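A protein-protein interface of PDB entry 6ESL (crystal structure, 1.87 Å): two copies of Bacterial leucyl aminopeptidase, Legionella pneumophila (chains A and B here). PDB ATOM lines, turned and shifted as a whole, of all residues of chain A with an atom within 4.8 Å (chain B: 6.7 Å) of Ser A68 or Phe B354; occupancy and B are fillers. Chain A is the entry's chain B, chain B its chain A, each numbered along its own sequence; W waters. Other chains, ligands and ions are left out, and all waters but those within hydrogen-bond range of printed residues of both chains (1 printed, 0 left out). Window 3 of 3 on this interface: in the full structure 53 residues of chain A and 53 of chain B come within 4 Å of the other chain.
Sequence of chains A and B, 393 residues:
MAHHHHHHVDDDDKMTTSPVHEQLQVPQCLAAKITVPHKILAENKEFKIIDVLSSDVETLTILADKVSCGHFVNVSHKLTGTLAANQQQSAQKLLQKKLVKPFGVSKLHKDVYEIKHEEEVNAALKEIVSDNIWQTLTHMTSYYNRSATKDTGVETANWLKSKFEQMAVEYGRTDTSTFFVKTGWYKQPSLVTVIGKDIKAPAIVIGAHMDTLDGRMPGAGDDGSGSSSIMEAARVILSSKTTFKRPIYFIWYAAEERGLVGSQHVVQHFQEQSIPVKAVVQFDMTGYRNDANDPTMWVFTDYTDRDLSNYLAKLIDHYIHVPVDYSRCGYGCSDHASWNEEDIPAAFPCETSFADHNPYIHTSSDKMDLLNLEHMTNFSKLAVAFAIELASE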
ATOM      1  N   ALA A  64     -10.551  -9.625 -15.674  1.00  0.00           N
ATOM      2  CA  ALA A  64      -9.551  -8.633 -15.743  1.00  0.00           C
ATOM      3  C   ALA A  64     -10.220  -7.236 -15.854  1.00  0.00           C
ATOM      4  O   ALA A  64      -9.653  -6.232 -15.347  1.00  0.00           O
ATOM      5  CB  ALA A  64      -8.604  -8.804 -16.962  1.00  0.00           C
ATOM      6  N   ASP A  65     -11.313  -7.163 -16.613  1.00  0.00           N
ATOM      7  CA  ASP A  65     -12.042  -5.888 -16.839  1.00  0.00           C
ATOM      8  C   ASP A  65     -12.511  -5.378 -15.467  1.00  0.00           C
ATOM      9  O   ASP A  65     -12.183  -4.239 -15.128  1.00  0.00           O
ATOM     10  CB  ASP A  65     -13.284  -6.085 -17.707  1.00  0.00           C
ATOM     11  CG  ASP A  65     -12.945  -6.387 -19.244  1.00  0.00           C
ATOM     12  OD1 ASP A  65     -11.805  -6.069 -19.730  1.00  0.00           O
ATOM     13  OD2 ASP A  65     -13.865  -6.920 -19.930  1.00  0.00           O
ATOM     14  N   LYS A  66     -13.093  -6.270 -14.664  1.00  0.00           N
ATOM     15  CA  LYS A  66     -13.580  -5.900 -13.349  1.00  0.00           C
ATOM     16  C   LYS A  66     -12.499  -5.586 -12.343  1.00  0.00           C
ATOM     17  O   LYS A  66     -12.637  -4.663 -11.626  1.00  0.00           O
ATOM     18  CB  LYS A  66     -14.532  -6.940 -12.762  1.00  0.00           C
ATOM     19  CG  LYS A  66     -15.795  -7.168 -13.588  1.00  0.00           C
ATOM     20  CD  LYS A  66     -16.755  -5.959 -13.720  1.00  0.00           C
ATOM     21  CE  LYS A  66     -18.023  -6.330 -14.509  1.00  0.00           C
ATOM     22  NZ  LYS A  66     -18.969  -5.178 -14.679  1.00  0.00           N
ATOM     23  N   VAL A  67     -11.448  -6.377 -12.265  1.00  0.00           N
ATOM     24  CA  VAL A  67     -10.387  -6.189 -11.296  1.00  0.00           C
ATOM     25  C   VAL A  67      -9.594  -4.924 -11.586  1.00  0.00           C
ATOM     26  O   VAL A  67      -9.102  -4.293 -10.651  1.00  0.00           O
ATOM     27  CB  VAL A  67      -9.490  -7.442 -11.184  1.00  0.00           C
ATOM     28  CG1 VAL A  67      -8.169  -7.106 -10.424  1.00  0.00           C
ATOM     29  CG2 VAL A  67     -10.277  -8.601 -10.594  1.00  0.00           C
ATOM     30  N   SER A  68      -9.521  -4.502 -12.852  1.00  0.00           N
ATOM     31  CA  SER A  68      -9.000  -3.225 -13.199  1.00  0.00           C
ATOM     32  C   SER A  68      -7.552  -2.996 -12.764  1.00  0.00           C
ATOM     33  O   SER A  68      -7.184  -1.852 -12.424  1.00  0.00           O
ATOM     34  CB  SER A  68      -9.951  -2.142 -12.594  1.00  0.00           C
ATOM     35  OG  SER A  68      -9.675  -0.898 -13.148  1.00  0.00           O
ATOM     36  N   CYS A  69      -6.693  -4.031 -12.794  1.00  0.00           N
ATOM     37  CA  CYS A  69      -5.283  -3.851 -12.558  1.00  0.00           C
ATOM     38  C   CYS A  69      -4.377  -4.299 -13.739  1.00  0.00           C
ATOM     39  O   CYS A  69      -3.146  -4.285 -13.637  1.00  0.00           O
ATOM     40  CB  CYS A  69      -4.963  -4.619 -11.275  1.00  0.00           C
ATOM     41  SG  CYS A  69      -4.748  -6.399 -11.484  1.00  0.00           S
ATOM     42  N   GLY A  70      -5.003  -4.592 -14.885  1.00  0.00           N
ATOM     43  CA  GLY A  70      -4.283  -5.038 -16.101  1.00  0.00           C
ATOM     44  C   GLY A  70      -4.933  -6.290 -16.714  1.00  0.00           C
ATOM     45  O   GLY A  70      -5.750  -6.960 -16.082  1.00  0.00           O
ATOM     46  N   LEU A 108      -2.500   1.201 -11.690  1.00  0.00           N
ATOM     47  CA  LEU A 108      -3.626   1.931 -12.363  1.00  0.00           C
ATOM     48  C   LEU A 108      -4.543   2.729 -11.419  1.00  0.00           C
ATOM     49  O   LEU A 108      -5.340   3.543 -11.900  1.00  0.00           O
ATOM     50  CB  LEU A 108      -4.473   0.919 -13.192  1.00  0.00           C
ATOM     51  CG  LEU A 108      -3.678  -0.003 -14.133  1.00  0.00           C
ATOM     52  CD1 LEU A 108      -4.689  -0.729 -15.006  1.00  0.00           C
ATOM     53  CD2 LEU A 108      -2.772   0.856 -15.004  1.00  0.00           C
ATOM     54  N   HIS A 109      -4.423   2.475 -10.118  1.00  0.00           N
ATOM     55  CA  HIS A 109      -5.270   3.164  -9.117  1.00  0.00           C
ATOM     56  C   HIS A 109      -4.423   3.921  -8.101  1.00  0.00           C
ATOM     57  O   HIS A 109      -4.886   4.189  -6.966  1.00  0.00           O
ATOM     58  CB  HIS A 109      -6.229   2.158  -8.500  1.00  0.00           C
ATOM     59  CG  HIS A 109      -7.048   1.488  -9.540  1.00  0.00           C
ATOM     60  ND1 HIS A 109      -8.063   2.142 -10.205  1.00  0.00           N
ATOM     61  CD2 HIS A 109      -6.916   0.287 -10.146  1.00  0.00           C
ATOM     62  CE1 HIS A 109      -8.588   1.342 -11.114  1.00  0.00           C
ATOM     63  NE2 HIS A 109      -7.907   0.214 -11.101  1.00  0.00           N
ATOM     64  N   TRP B 298      -6.385  11.174 -25.620  1.00  0.00           N
ATOM     65  CA  TRP B 298      -5.579  10.661 -24.523  1.00  0.00           C
ATOM     66  C   TRP B 298      -4.407   9.896 -25.060  1.00  0.00           C
ATOM     67  O   TRP B 298      -4.562   9.115 -25.993  1.00  0.00           O
ATOM     68  CB  TRP B 298      -6.478   9.782 -23.618  1.00  0.00           C
ATOM     69  CG  TRP B 298      -7.510  10.597 -22.909  1.00  0.00           C
ATOM     70  CD1 TRP B 298      -8.717  10.971 -23.391  1.00  0.00           C
ATOM     71  CD2 TRP B 298      -7.438  11.112 -21.551  1.00  0.00           C
ATOM     72  NE1 TRP B 298      -9.386  11.703 -22.442  1.00  0.00           N
ATOM     73  CE2 TRP B 298      -8.647  11.760 -21.303  1.00  0.00           C
ATOM     74  CE3 TRP B 298      -6.515  10.992 -20.513  1.00  0.00           C
ATOM     75  CZ2 TRP B 298      -8.930  12.392 -20.084  1.00  0.00           C
ATOM     76  CZ3 TRP B 298      -6.826  11.587 -19.275  1.00  0.00           C
ATOM     77  CH2 TRP B 298      -8.025  12.284 -19.089  1.00  0.00           C
ATOM     78  N   PHE B 300      -1.577   7.220 -24.059  1.00  0.00           N
ATOM     79  CA  PHE B 300      -1.282   6.245 -23.017  1.00  0.00           C
ATOM     80  C   PHE B 300       0.222   6.087 -22.754  1.00  0.00           C
ATOM     81  O   PHE B 300       1.004   6.046 -23.648  1.00  0.00           O
ATOM     82  CB  PHE B 300      -2.014   4.920 -23.274  1.00  0.00           C
ATOM     83  CG  PHE B 300      -3.419   5.000 -22.792  1.00  0.00           C
ATOM     84  CD1 PHE B 300      -4.332   5.826 -23.462  1.00  0.00           C
ATOM     85  CD2 PHE B 300      -3.796   4.485 -21.585  1.00  0.00           C
ATOM     86  CE1 PHE B 300      -5.653   6.033 -22.949  1.00  0.00           C
ATOM     87  CE2 PHE B 300      -5.102   4.652 -21.092  1.00  0.00           C
ATOM     88  CZ  PHE B 300      -6.064   5.375 -21.814  1.00  0.00           C
ATOM     89  N   SER B 327      -2.849   8.948 -19.608  1.00  0.00           N
ATOM     90  CA  SER B 327      -3.391   7.891 -18.807  1.00  0.00           C
ATOM     91  C   SER B 327      -2.588   6.604 -18.982  1.00  0.00           C
ATOM     92  O   SER B 327      -1.704   6.562 -19.771  1.00  0.00           O
ATOM     93  CB  SER B 327      -4.856   7.684 -19.144  1.00  0.00           C
ATOM     94  OG  SER B 327      -5.482   6.720 -18.348  1.00  0.00           O
ATOM     95  N   ARG B 328      -2.879   5.611 -18.162  1.00  0.00           N
ATOM     96  CA  ARG B 328      -2.259   4.287 -18.211  1.00  0.00           C
ATOM     97  C   ARG B 328      -3.365   3.251 -18.330  1.00  0.00           C
ATOM     98  O   ARG B 328      -4.398   3.433 -17.741  1.00  0.00           O
ATOM     99  CB  ARG B 328      -1.525   3.971 -16.916  1.00  0.00           C
ATOM    100  CG  ARG B 328      -0.364   4.854 -16.495  1.00  0.00           C
ATOM    101  CD  ARG B 328       0.136   4.427 -15.116  1.00  0.00           C
ATOM    102  NE  ARG B 328       1.306   5.144 -14.679  1.00  0.00           N
ATOM    103  CZ  ARG B 328       1.925   4.961 -13.524  1.00  0.00           C
ATOM    104  NH1 ARG B 328       2.999   5.656 -13.234  1.00  0.00           N
ATOM    105  NH2 ARG B 328       1.488   4.079 -12.656  1.00  0.00           N
ATOM    106  N   CYS B 329      -3.169   2.197 -19.126  1.00  0.00           N
ATOM    107  CA  CYS B 329      -4.164   1.151 -19.226  1.00  0.00           C
ATOM    108  C   CYS B 329      -3.755  -0.265 -18.803  1.00  0.00           C
ATOM    109  O   CYS B 329      -4.510  -1.158 -18.919  1.00  0.00           O
ATOM    110  CB  CYS B 329      -4.850   1.137 -20.585  1.00  0.00           C
ATOM    111  SG  CYS B 329      -3.732   0.929 -21.922  1.00  0.00           S
ATOM    112  N   GLY B 330      -2.557  -0.442 -18.328  1.00  0.00           N
ATOM    113  CA  GLY B 330      -2.146  -1.713 -17.814  1.00  0.00           C
ATOM    114  C   GLY B 330      -1.502  -2.734 -18.695  1.00  0.00           C
ATOM    115  O   GLY B 330      -1.407  -2.596 -19.863  1.00  0.00           O
ATOM    116  N   CYS B 333      -2.532  -4.270 -22.593  1.00  0.00           N
ATOM    117  CA  CYS B 333      -3.637  -3.353 -22.798  1.00  0.00           C
ATOM    118  C   CYS B 333      -4.153  -3.393 -24.262  1.00  0.00           C
ATOM    119  O   CYS B 333      -5.332  -3.411 -24.510  1.00  0.00           O
ATOM    120  CB  CYS B 333      -3.119  -1.933 -22.549  1.00  0.00           C
ATOM    121  SG  CYS B 333      -4.445  -0.717 -22.895  1.00  0.00           S
ATOM    122  N   THR B 352     -10.575   7.874 -24.512  1.00  0.00           N
ATOM    123  CA  THR B 352     -10.823   8.335 -23.132  1.00  0.00           C
ATOM    124  C   THR B 352      -9.644   7.959 -22.283  1.00  0.00           C
ATOM    125  O   THR B 352      -8.797   7.165 -22.670  1.00  0.00           O
ATOM    126  CB  THR B 352     -12.058   7.636 -22.460  1.00  0.00           C
ATOM    127  OG1 THR B 352     -11.825   6.241 -22.433  1.00  0.00           O
ATOM    128  CG2 THR B 352     -13.349   7.736 -23.284  1.00  0.00           C
ATOM    129  N   SER B 353      -9.656   8.447 -21.058  1.00  0.00           N
ATOM    130  CA  SER B 353      -8.791   7.873 -20.073  1.00  0.00           C
ATOM    131  C   SER B 353      -9.244   6.437 -19.761  1.00  0.00           C
ATOM    132  O   SER B 353     -10.404   6.028 -20.035  1.00  0.00           O
ATOM    133  CB  SER B 353      -8.823   8.695 -18.770  1.00  0.00           C
ATOM    134  OG  SER B 353     -10.053   8.492 -18.131  1.00  0.00           O
ATOM    135  N   PHE B 354      -8.391   5.732 -19.048  1.00  0.00           N
ATOM    136  CA  PHE B 354      -8.737   4.430 -18.472  1.00  0.00           C
ATOM    137  C   PHE B 354      -9.821   4.480 -17.427  1.00  0.00           C
ATOM    138  O   PHE B 354     -10.775   3.719 -17.500  1.00  0.00           O
ATOM    139  CB  PHE B 354      -7.500   3.785 -17.907  1.00  0.00           C
ATOM    140  CG  PHE B 354      -7.745   2.464 -17.291  1.00  0.00           C
ATOM    141  CD1 PHE B 354      -7.889   1.331 -18.101  1.00  0.00           C
ATOM    142  CD2 PHE B 354      -7.817   2.338 -15.877  1.00  0.00           C
ATOM    143  CE1 PHE B 354      -8.144   0.086 -17.535  1.00  0.00           C
ATOM    144  CE2 PHE B 354      -8.025   1.057 -15.319  1.00  0.00           C
ATOM    145  CZ  PHE B 354      -8.198  -0.044 -16.168  1.00  0.00           C
ATOM    146  N   ALA B 355      -9.776   5.438 -16.534  1.00  0.00           N
ATOM    147  CA  ALA B 355     -10.826   5.569 -15.539  1.00  0.00           C
ATOM    148  C   ALA B 355     -12.208   5.846 -16.134  1.00  0.00           C
ATOM    149  O   ALA B 355     -13.198   5.348 -15.655  1.00  0.00           O
ATOM    150  CB  ALA B 355     -10.457   6.615 -14.519  1.00  0.00           C
ATOM    151  N   ASP B 356     -12.276   6.616 -17.194  1.00  0.00           N
ATOM    152  CA  ASP B 356     -13.548   6.940 -17.806  1.00  0.00           C
ATOM    153  C   ASP B 356     -13.836   6.219 -19.098  1.00  0.00           C
ATOM    154  O   ASP B 356     -14.406   6.772 -19.970  1.00  0.00           O
ATOM    155  CB  ASP B 356     -13.677   8.426 -18.067  1.00  0.00           C
ATOM    156  CG  ASP B 356     -13.668   9.218 -16.841  1.00  0.00           C
ATOM    157  OD1 ASP B 356     -14.465   8.948 -15.971  1.00  0.00           O
ATOM    158  OD2 ASP B 356     -12.848  10.115 -16.763  1.00  0.00           O
ATOM    159  N   HIS B 357     -13.429   4.982 -19.228  1.00  0.00           N
ATOM    160  CA  HIS B 357     -13.647   4.299 -20.473  1.00  0.00           C
ATOM    161  C   HIS B 357     -15.085   3.913 -20.781  1.00  0.00           C
ATOM    162  O   HIS B 357     -15.919   3.896 -19.939  1.00  0.00           O
ATOM    163  CB  HIS B 357     -12.688   3.171 -20.644  1.00  0.00           C
ATOM    164  CG  HIS B 357     -12.922   2.046 -19.723  1.00  0.00           C
ATOM    165  ND1 HIS B 357     -14.003   1.218 -19.837  1.00  0.00           N
ATOM    166  CD2 HIS B 357     -12.179   1.561 -18.716  1.00  0.00           C
ATOM    167  CE1 HIS B 357     -13.941   0.284 -18.915  1.00  0.00           C
ATOM    168  NE2 HIS B 357     -12.842   0.474 -18.213  1.00  0.00           N
ATOM    169  N   ASN B 358     -15.330   3.645 -22.043  1.00  0.00           N
ATOM    170  CA  ASN B 358     -16.668   3.332 -22.564  1.00  0.00           C
ATOM    171  C   ASN B 358     -17.193   2.140 -21.695  1.00  0.00           C
ATOM    172  O   ASN B 358     -16.589   1.048 -21.730  1.00  0.00           O
ATOM    173  CB  ASN B 358     -16.494   2.887 -24.028  1.00  0.00           C
ATOM    174  CG  ASN B 358     -17.773   2.484 -24.697  1.00  0.00           C
ATOM    175  OD1 ASN B 358     -18.780   2.338 -24.007  1.00  0.00           O
ATOM    176  ND2 ASN B 358     -17.740   2.243 -26.019  1.00  0.00           N
HETATM  177  O   HOH W   1      -4.854   4.626 -15.192  1.00  0.00           O
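Among the printed residues, pairs that only touch across the chains: Ser A68 with Phe B354, Leu A108 with Gly B330, Leu A108 with Phe B354, Leu A108 with Arg B328 and Leu A108 with Cys B329.
The backbone NH (N) of Phe B354 is in hydrogen-bond range of the side-chain hydroxyl (OG) of Ser B327 (3.2 Å). SG of Cys B329 forms a disulfide with SG of Cys B333, at 2.0 Å. The backbone carbonyl oxygen (O) of Ser A68 is in hydrogen-bond range of a ring nitrogen (NE2) of His A109 (2.6 Å).
No position is printed for both chains. Of the 5 pairs that touch across the chains among the printed residues, none has its exchanged pair printed and touching as well.
Water W1 bridges O of Arg B328 (2.9 Å) and O of Leu A108 (3.5 Å).
Hydrophobic or aromatic side chains of chain B that line the printed part of chain A: Phe B354. Of the 9 printed residues of chain A, 2 touch a printed residue of chain B. Printed residues of chain A that touch a printed residue of chain B: Ser A68 and Leu A108. Hydrophobic or aromatic side chains of chain A that line the printed part of chain B: Leu A108. Among the printed residues, 5 pairs touch across the chains. Among the printed residues, no Asp or Glu carboxylate lies within 4 Å of a Lys or Arg side-chain nitrogen of the other chain.
Ser A68 touches just one residue of chain B: Phe B354 (3.4 Å). Printed residues of chain B within 4 Å of Leu A108: Arg B328 (3.9 Å), Cys B329 (3.9 Å), Gly B330 (3.6 Å) and Phe B354 (3.8 Å). Of the printed residues of chain A, Arg B328 touches Leu A108. Printed residues of chain A within 4 Å of Cys B329: Leu A108 (3.9 Å). Of the printed residues of chain A, Gly B330 touches Leu A108 (3.6 Å). Phe B354 touches just these residues of chain A: Ser A68 (3.4 Å) and Leu A108 (3.8 Å).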
